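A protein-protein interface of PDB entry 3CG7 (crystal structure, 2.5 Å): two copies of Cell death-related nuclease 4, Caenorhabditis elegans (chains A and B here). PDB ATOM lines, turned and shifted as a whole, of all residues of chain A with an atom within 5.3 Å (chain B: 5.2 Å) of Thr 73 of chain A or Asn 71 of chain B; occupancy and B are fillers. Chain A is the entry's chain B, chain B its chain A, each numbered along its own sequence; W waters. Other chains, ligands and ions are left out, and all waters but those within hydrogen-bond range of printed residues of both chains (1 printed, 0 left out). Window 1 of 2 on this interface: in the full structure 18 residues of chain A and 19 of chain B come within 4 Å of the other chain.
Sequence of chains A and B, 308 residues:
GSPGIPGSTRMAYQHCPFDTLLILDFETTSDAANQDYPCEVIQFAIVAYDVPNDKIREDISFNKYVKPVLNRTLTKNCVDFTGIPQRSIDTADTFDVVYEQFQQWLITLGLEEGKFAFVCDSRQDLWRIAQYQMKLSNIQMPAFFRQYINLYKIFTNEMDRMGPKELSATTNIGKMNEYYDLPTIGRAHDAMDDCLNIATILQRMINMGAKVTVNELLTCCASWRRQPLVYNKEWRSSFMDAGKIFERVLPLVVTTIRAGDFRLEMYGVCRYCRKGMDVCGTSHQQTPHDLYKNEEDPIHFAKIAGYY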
ATOM      1  N   LEU A  70       1.272   8.217  25.720  1.00  0.00           N
ATOM      2  CA  LEU A  70       0.908   9.240  24.743  1.00  0.00           C
ATOM      3  C   LEU A  70      -0.429   8.942  24.080  1.00  0.00           C
ATOM      4  O   LEU A  70      -1.252   9.840  23.903  1.00  0.00           O
ATOM      5  CB  LEU A  70       2.012   9.419  23.696  1.00  0.00           C
ATOM      6  CG  LEU A  70       3.097  10.497  23.856  1.00  0.00           C
ATOM      7  CD1 LEU A  70       3.475  10.838  25.302  1.00  0.00           C
ATOM      8  CD2 LEU A  70       4.335  10.094  23.048  1.00  0.00           C
ATOM      9  N   ASN A  71      -0.636   7.684  23.708  1.00  0.00           N
ATOM     10  CA  ASN A  71      -1.886   7.249  23.093  1.00  0.00           C
ATOM     11  C   ASN A  71      -2.423   6.014  23.810  1.00  0.00           C
ATOM     12  O   ASN A  71      -2.143   4.875  23.430  1.00  0.00           O
ATOM     13  CB  ASN A  71      -1.704   7.029  21.592  1.00  0.00           C
ATOM     14  CG  ASN A  71      -1.497   8.335  20.839  1.00  0.00           C
ATOM     15  OD1 ASN A  71      -0.435   8.572  20.253  1.00  0.00           O
ATOM     16  ND2 ASN A  71      -2.506   9.201  20.871  1.00  0.00           N
ATOM     17  N   ARG A  72      -3.202   6.280  24.856  1.00  0.00           N
ATOM     18  CA  ARG A  72      -3.627   5.279  25.831  1.00  0.00           C
ATOM     19  C   ARG A  72      -4.673   4.287  25.333  1.00  0.00           C
ATOM     20  O   ARG A  72      -4.778   3.180  25.847  1.00  0.00           O
ATOM     21  CB  ARG A  72      -4.079   5.974  27.118  1.00  0.00           C
ATOM     22  CG  ARG A  72      -2.975   6.017  28.145  1.00  0.00           C
ATOM     23  CD  ARG A  72      -3.195   7.026  29.241  1.00  0.00           C
ATOM     24  NE  ARG A  72      -2.438   8.246  28.976  1.00  0.00           N
ATOM     25  CZ  ARG A  72      -2.072   9.122  29.910  1.00  0.00           C
ATOM     26  NH1 ARG A  72      -2.390   8.914  31.185  1.00  0.00           N
ATOM     27  NH2 ARG A  72      -1.377  10.203  29.568  1.00  0.00           N
ATOM     28  N   THR A  73      -5.408   4.675  24.306  1.00  0.00           N
ATOM     29  CA  THR A  73      -6.451   3.846  23.734  1.00  0.00           C
ATOM     30  C   THR A  73      -5.966   3.330  22.402  1.00  0.00           C
ATOM     31  O   THR A  73      -5.589   4.107  21.530  1.00  0.00           O
ATOM     32  CB  THR A  73      -7.759   4.651  23.546  1.00  0.00           C
ATOM     33  OG1 THR A  73      -8.115   5.245  24.795  1.00  0.00           O
ATOM     34  CG2 THR A  73      -8.899   3.764  23.066  1.00  0.00           C
ATOM     35  N   LEU A  74      -5.972   2.009  22.273  1.00  0.00           N
ATOM     36  CA  LEU A  74      -5.532   1.332  21.072  1.00  0.00           C
ATOM     37  C   LEU A  74      -6.523   1.546  19.956  1.00  0.00           C
ATOM     38  O   LEU A  74      -7.721   1.347  20.106  1.00  0.00           O
ATOM     39  CB  LEU A  74      -5.345  -0.167  21.326  1.00  0.00           C
ATOM     40  CG  LEU A  74      -3.946  -0.763  21.533  1.00  0.00           C
ATOM     41  CD1 LEU A  74      -2.943   0.219  22.135  1.00  0.00           C
ATOM     42  CD2 LEU A  74      -4.028  -2.051  22.362  1.00  0.00           C
ATOM     43  N   THR A  75      -5.988   1.981  18.837  1.00  0.00           N
ATOM     44  CA  THR A  75      -6.711   2.096  17.600  1.00  0.00           C
ATOM     45  C   THR A  75      -7.269   0.733  17.180  1.00  0.00           C
ATOM     46  O   THR A  75      -6.655  -0.304  17.445  1.00  0.00           O
ATOM     47  CB  THR A  75      -5.738   2.654  16.561  1.00  0.00           C
ATOM     48  OG1 THR A  75      -5.884   4.082  16.502  1.00  0.00           O
ATOM     49  CG2 THR A  75      -5.968   2.077  15.228  1.00  0.00           C
ATOM     50  N   GLN A  86      -7.460  -4.295  24.395  1.00  0.00           N
ATOM     51  CA  GLN A  86      -7.316  -3.129  25.278  1.00  0.00           C
ATOM     52  C   GLN A  86      -7.070  -3.469  26.750  1.00  0.00           C
ATOM     53  O   GLN A  86      -6.232  -2.837  27.397  1.00  0.00           O
ATOM     54  CB  GLN A  86      -8.525  -2.189  25.146  1.00  0.00           C
ATOM     55  CG  GLN A  86      -8.369  -0.862  25.891  1.00  0.00           C
ATOM     56  CD  GLN A  86      -7.323   0.042  25.252  1.00  0.00           C
ATOM     57  OE1 GLN A  86      -7.344   0.268  24.041  1.00  0.00           O
ATOM     58  NE2 GLN A  86      -6.404   0.565  26.067  1.00  0.00           N
ATOM     59  N   THR B  29     -11.788  13.808  20.232  1.00  0.00           N
ATOM     60  CA  THR B  29     -11.056  12.631  19.770  1.00  0.00           C
ATOM     61  C   THR B  29     -12.042  11.489  19.535  1.00  0.00           C
ATOM     62  O   THR B  29     -13.072  11.389  20.221  1.00  0.00           O
ATOM     63  CB  THR B  29     -10.009  12.169  20.810  1.00  0.00           C
ATOM     64  OG1 THR B  29     -10.653  11.915  22.066  1.00  0.00           O
ATOM     65  CG2 THR B  29      -8.920  13.229  21.011  1.00  0.00           C
ATOM     66  N   ASN B  34     -14.595   2.108  16.835  1.00  0.00           N
ATOM     67  CA  ASN B  34     -14.573   1.752  18.246  1.00  0.00           C
ATOM     68  C   ASN B  34     -15.309   2.759  19.115  1.00  0.00           C
ATOM     69  O   ASN B  34     -14.932   3.932  19.213  1.00  0.00           O
ATOM     70  CB  ASN B  34     -13.145   1.585  18.760  1.00  0.00           C
ATOM     71  CG  ASN B  34     -13.101   1.199  20.226  1.00  0.00           C
ATOM     72  OD1 ASN B  34     -13.939   0.420  20.702  1.00  0.00           O
ATOM     73  ND2 ASN B  34     -12.134   1.743  20.953  1.00  0.00           N
ATOM     74  N   ASP B  36     -15.883   2.183  22.438  1.00  0.00           N
ATOM     75  CA  ASP B  36     -15.357   2.118  23.804  1.00  0.00           C
ATOM     76  C   ASP B  36     -14.130   3.017  23.838  1.00  0.00           C
ATOM     77  O   ASP B  36     -12.983   2.552  23.882  1.00  0.00           O
ATOM     78  CB  ASP B  36     -15.023   0.673  24.207  1.00  0.00           C
ATOM     79  CG  ASP B  36     -14.653   0.529  25.691  1.00  0.00           C
ATOM     80  OD1 ASP B  36     -14.618   1.543  26.422  1.00  0.00           O
ATOM     81  OD2 ASP B  36     -14.385  -0.617  26.129  1.00  0.00           O
ATOM     82  N   TYR B  37     -14.398   4.317  23.798  1.00  0.00           N
ATOM     83  CA  TYR B  37     -13.380   5.313  23.546  1.00  0.00           C
ATOM     84  C   TYR B  37     -13.501   6.473  24.524  1.00  0.00           C
ATOM     85  O   TYR B  37     -14.590   7.003  24.729  1.00  0.00           O
ATOM     86  CB  TYR B  37     -13.485   5.807  22.105  1.00  0.00           C
ATOM     87  CG  TYR B  37     -12.257   6.559  21.638  1.00  0.00           C
ATOM     88  CD1 TYR B  37     -11.211   5.892  20.983  1.00  0.00           C
ATOM     89  CD2 TYR B  37     -12.132   7.935  21.856  1.00  0.00           C
ATOM     90  CE1 TYR B  37     -10.086   6.569  20.563  1.00  0.00           C
ATOM     91  CE2 TYR B  37     -10.994   8.625  21.436  1.00  0.00           C
ATOM     92  CZ  TYR B  37      -9.977   7.939  20.787  1.00  0.00           C
ATOM     93  OH  TYR B  37      -8.854   8.630  20.367  1.00  0.00           O
ATOM     94  N   PRO B  38     -12.377   6.880  25.129  1.00  0.00           N
ATOM     95  CA  PRO B  38     -12.420   7.977  26.070  1.00  0.00           C
ATOM     96  C   PRO B  38     -12.372   9.321  25.338  1.00  0.00           C
ATOM     97  O   PRO B  38     -11.322   9.965  25.288  1.00  0.00           O
ATOM     98  CB  PRO B  38     -11.152   7.766  26.895  1.00  0.00           C
ATOM     99  CG  PRO B  38     -10.207   7.091  25.988  1.00  0.00           C
ATOM    100  CD  PRO B  38     -11.010   6.364  24.947  1.00  0.00           C
ATOM    101  N   GLU B  40     -12.159  12.921  24.203  1.00  0.00           N
ATOM    102  CA  GLU B  40     -11.641  14.151  24.786  1.00  0.00           C
ATOM    103  C   GLU B  40     -11.956  15.326  23.875  1.00  0.00           C
ATOM    104  O   GLU B  40     -11.873  15.197  22.652  1.00  0.00           O
ATOM    105  CB  GLU B  40     -10.134  14.048  25.005  1.00  0.00           C
ATOM    106  CG  GLU B  40      -9.735  13.256  26.238  1.00  0.00           C
ATOM    107  CD  GLU B  40      -8.232  13.036  26.310  1.00  0.00           C
ATOM    108  OE1 GLU B  40      -7.704  12.231  25.501  1.00  0.00           O
ATOM    109  OE2 GLU B  40      -7.582  13.678  27.171  1.00  0.00           O
ATOM    110  N   PRO B  68      -5.740  17.162  23.978  1.00  0.00           N
ATOM    111  CA  PRO B  68      -6.067  15.995  24.799  1.00  0.00           C
ATOM    112  C   PRO B  68      -4.842  15.446  25.530  1.00  0.00           C
ATOM    113  O   PRO B  68      -3.706  15.729  25.135  1.00  0.00           O
ATOM    114  CB  PRO B  68      -6.584  14.981  23.783  1.00  0.00           C
ATOM    115  CG  PRO B  68      -6.014  15.403  22.479  1.00  0.00           C
ATOM    116  CD  PRO B  68      -5.762  16.863  22.536  1.00  0.00           C
ATOM    117  N   VAL B  69      -5.074  14.690  26.601  1.00  0.00           N
ATOM    118  CA  VAL B  69      -3.975  14.099  27.362  1.00  0.00           C
ATOM    119  C   VAL B  69      -3.904  12.573  27.215  1.00  0.00           C
ATOM    120  O   VAL B  69      -2.814  12.009  27.226  1.00  0.00           O
ATOM    121  CB  VAL B  69      -3.939  14.567  28.878  1.00  0.00           C
ATOM    122  CG1 VAL B  69      -4.001  16.082  28.977  1.00  0.00           C
ATOM    123  CG2 VAL B  69      -5.057  13.948  29.704  1.00  0.00           C
ATOM    124  N   LEU B  70      -5.047  11.913  27.047  1.00  0.00           N
ATOM    125  CA  LEU B  70      -5.083  10.451  26.948  1.00  0.00           C
ATOM    126  C   LEU B  70      -4.733   9.929  25.550  1.00  0.00           C
ATOM    127  O   LEU B  70      -4.048   8.910  25.402  1.00  0.00           O
ATOM    128  CB  LEU B  70      -6.451   9.905  27.368  1.00  0.00           C
ATOM    129  CG  LEU B  70      -7.107  10.333  28.688  1.00  0.00           C
ATOM    130  CD1 LEU B  70      -8.497   9.704  28.760  1.00  0.00           C
ATOM    131  CD2 LEU B  70      -6.279   9.957  29.933  1.00  0.00           C
ATOM    132  N   ASN B  71      -5.237  10.601  24.526  1.00  0.00           N
ATOM    133  CA  ASN B  71      -4.904  10.244  23.159  1.00  0.00           C
ATOM    134  C   ASN B  71      -4.440  11.480  22.413  1.00  0.00           C
ATOM    135  O   ASN B  71      -5.242  12.221  21.835  1.00  0.00           O
ATOM    136  CB  ASN B  71      -6.070   9.543  22.472  1.00  0.00           C
ATOM    137  CG  ASN B  71      -6.350   8.173  23.067  1.00  0.00           C
ATOM    138  OD1 ASN B  71      -7.329   7.993  23.792  1.00  0.00           O
ATOM    139  ND2 ASN B  71      -5.481   7.204  22.781  1.00  0.00           N
ATOM    140  N   ARG B  72      -3.131  11.702  22.460  1.00  0.00           N
ATOM    141  CA  ARG B  72      -2.536  12.957  22.024  1.00  0.00           C
ATOM    142  C   ARG B  72      -2.441  13.074  20.508  1.00  0.00           C
ATOM    143  O   ARG B  72      -2.329  14.175  19.981  1.00  0.00           O
ATOM    144  CB  ARG B  72      -1.181  13.169  22.705  1.00  0.00           C
ATOM    145  CG  ARG B  72      -1.271  13.130  24.242  1.00  0.00           C
ATOM    146  CD  ARG B  72      -0.073  13.792  24.920  1.00  0.00           C
ATOM    147  NE  ARG B  72       0.270  15.058  24.249  1.00  0.00           N
ATOM    148  CZ  ARG B  72       1.378  15.771  24.468  1.00  0.00           C
ATOM    149  NH1 ARG B  72       2.279  15.373  25.366  1.00  0.00           N
ATOM    150  NH2 ARG B  72       1.574  16.895  23.779  1.00  0.00           N
ATOM    151  N   THR B  73      -2.523  11.938  19.817  1.00  0.00           N
ATOM    152  CA  THR B  73      -2.454  11.880  18.355  1.00  0.00           C
ATOM    153  C   THR B  73      -3.826  11.564  17.787  1.00  0.00           C
ATOM    154  O   THR B  73      -4.399  10.526  18.094  1.00  0.00           O
ATOM    155  CB  THR B  73      -1.462  10.778  17.885  1.00  0.00           C
ATOM    156  OG1 THR B  73      -0.227  10.928  18.589  1.00  0.00           O
ATOM    157  CG2 THR B  73      -1.199  10.843  16.375  1.00  0.00           C
ATOM    158  N   LEU B  74      -4.353  12.451  16.955  1.00  0.00           N
ATOM    159  CA  LEU B  74      -5.655  12.214  16.348  1.00  0.00           C
ATOM    160  C   LEU B  74      -5.558  11.081  15.351  1.00  0.00           C
ATOM    161  O   LEU B  74      -4.597  11.014  14.587  1.00  0.00           O
ATOM    162  CB  LEU B  74      -6.168  13.464  15.645  1.00  0.00           C
ATOM    163  CG  LEU B  74      -6.315  14.765  16.440  1.00  0.00           C
ATOM    164  CD1 LEU B  74      -6.962  15.813  15.557  1.00  0.00           C
ATOM    165  CD2 LEU B  74      -7.120  14.557  17.706  1.00  0.00           C
ATOM    166  N   HIS B 300     -13.411  -0.065  28.784  1.00  0.00           N
ATOM    167  CA  HIS B 300     -12.199   0.750  28.740  1.00  0.00           C
ATOM    168  C   HIS B 300     -12.435   2.210  29.159  1.00  0.00           C
ATOM    169  O   HIS B 300     -11.710   2.723  30.009  1.00  0.00           O
ATOM    170  CB  HIS B 300     -11.520   0.667  27.369  1.00  0.00           C
ATOM    171  CG  HIS B 300     -10.420   1.665  27.182  1.00  0.00           C
ATOM    172  ND1 HIS B 300      -9.336   1.748  28.031  1.00  0.00           N
ATOM    173  CD2 HIS B 300     -10.237   2.627  26.244  1.00  0.00           C
ATOM    174  CE1 HIS B 300      -8.535   2.717  27.628  1.00  0.00           C
ATOM    175  NE2 HIS B 300      -9.056   3.262  26.541  1.00  0.00           N
HETATM  176  O   HOH W   1      -0.064  12.361  28.036  1.00  0.00           O
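Thr 73 of chain A touches just these residues of chain B: Tyr 37, Pro 38, Asn 71 and His 300. Thr 75 of chain A touches none of the printed residues of chain B. Printed residues of chain A within 4 Å of Leu 70 of chain B: Leu 70 (3.3 Å), Asn 71 (3.6 Å) and Arg 72 (2.8 Å). Printed residues of chain A within 4 Å of Arg 72 of chain B: Leu 70 (3.0 Å) and Asn 71 (3.0 Å). Leu 74 of chain B touches none of the printed residues of chain A. The nearest printed residue of chain B that does not touch Thr 73 of chain A is Asp 36 of chain B (4.3 Å). The nearest residue of chain A that does not touch Asn 71 of chain B is Leu 74 of chain A (5.2 Å). The nearest printed residue of chain A that does not touch His 300 of chain B is Arg 72 of chain A (4.2 Å).
Water W1 bridges O of Val 69 of chain B (2.9 Å) and NH2 of Arg 72 of chain A (3.0 Å).
Of the 14 printed residues of chain B, 8 touch a printed residue of chain A. Hydrophobic or aromatic side chains of chain B within 4 Å of the printed part of chain A: Tyr 37, Pro 38 and His 300. Along chain B the printed residues that touch a printed residue of chain A span positions 37 to 300. Among the printed residues, no Asp or Glu carboxylate lies within 4 Å of a Lys or Arg side-chain nitrogen of the other chain.
N of Arg 72 of chain B lies close to ND2 of Asn 71 of chain A (3.0 Å). O of Leu 70 of chain B is in hydrogen-bond range of N of Arg 72 of chain A. The side-chain hydroxyl (OG1) of Thr 73 of chain B sits at hydrogen-bond distance from the side-chain amide oxygen (OD1) of Asn 71 of chain A, 2.9 Å away. ND2 of Asn 71 of chain B lies close to N of Arg 72 of chain A. The side-chain hydroxyl of Thr 73 of chain A lies within hydrogen-bond range of a ring nitrogen (NE2) of His 300 of chain B (2.8 Å). N of Arg 72 of chain B is in hydrogen-bond range of O of Leu 70 of chain A, 3.0 Å away. The backbone NH of Thr 73 of chain A sits close to the side-chain amide nitrogen of Asn 71 of chain B, at 3.0 Å. The backbone carbonyl oxygen (O) of Val 69 of chain B sits at hydrogen-bond distance from the guanidinium group (NH2) of Arg 72 of chain A, 3.3 Å away. The backbone carbonyl oxygen (O) of Leu 70 of chain B lies close to the backbone carbonyl oxygen (O) of Leu 70 of chain A (3.3 Å).
Among the printed residues, pairs that only touch across the chains: Leu 70 of chain A with Asn 71 of chain B (3.7 Å), Asn 71 of chain A with Leu 70 of chain B (3.6 Å), Asn 71 of chain A with Asn 71 of chain B (3.4 Å), Thr 73 of chain A with Tyr 37 of chain B (3.8 Å), Thr 73 of chain A with Pro 38 of chain B (3.0 Å) and Gln 86 of chain A with His 300 of chain B (3.4 Å).
The backbone NH (N) of His 300 of chain B lies within hydrogen-bond range of the side-chain carboxylate (OD2) of Asp 36 of chain B (2.9 Å). N of Val 69 of chain B sits at hydrogen-bond distance from OE2 of Glu 40 of chain B, 2.8 Å away. OE1 of Glu 40 of chain B sits at hydrogen-bond distance from N of Asn 71 of chain B (3.1 Å). The backbone NH (N) of Leu 74 of chain A lies within hydrogen-bond range of the side-chain amide oxygen (OE1) of Gln 86 of chain A (2.8 Å). The backbone carbonyl oxygen (O) of Arg 72 of chain A is in hydrogen-bond range of the side-chain amide nitrogen (NE2) of Gln 86 of chain A, 3.1 Å away. The backbone NH of Leu 70 of chain B lies within hydrogen-bond range of the side-chain carboxylate of Glu 40 of chain B (3.1 Å).
Leu 70 of chain A touches its own counterpart, Leu 70 of chain B. Leu 70 of chain A touches Arg 72 of chain B, and with the chains exchanged Arg 72 of chain A touches Leu 70 of chain B. Asn 71 of chain A touches its own counterpart, Asn 71 of chain B. Asn 71 of chain A touches Arg 72 of chain B, and with the chains exchanged Arg 72 of chain A touches Asn 71 of chain B. Positions printed for both chains: 70, 71, 72, 73 and 74.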
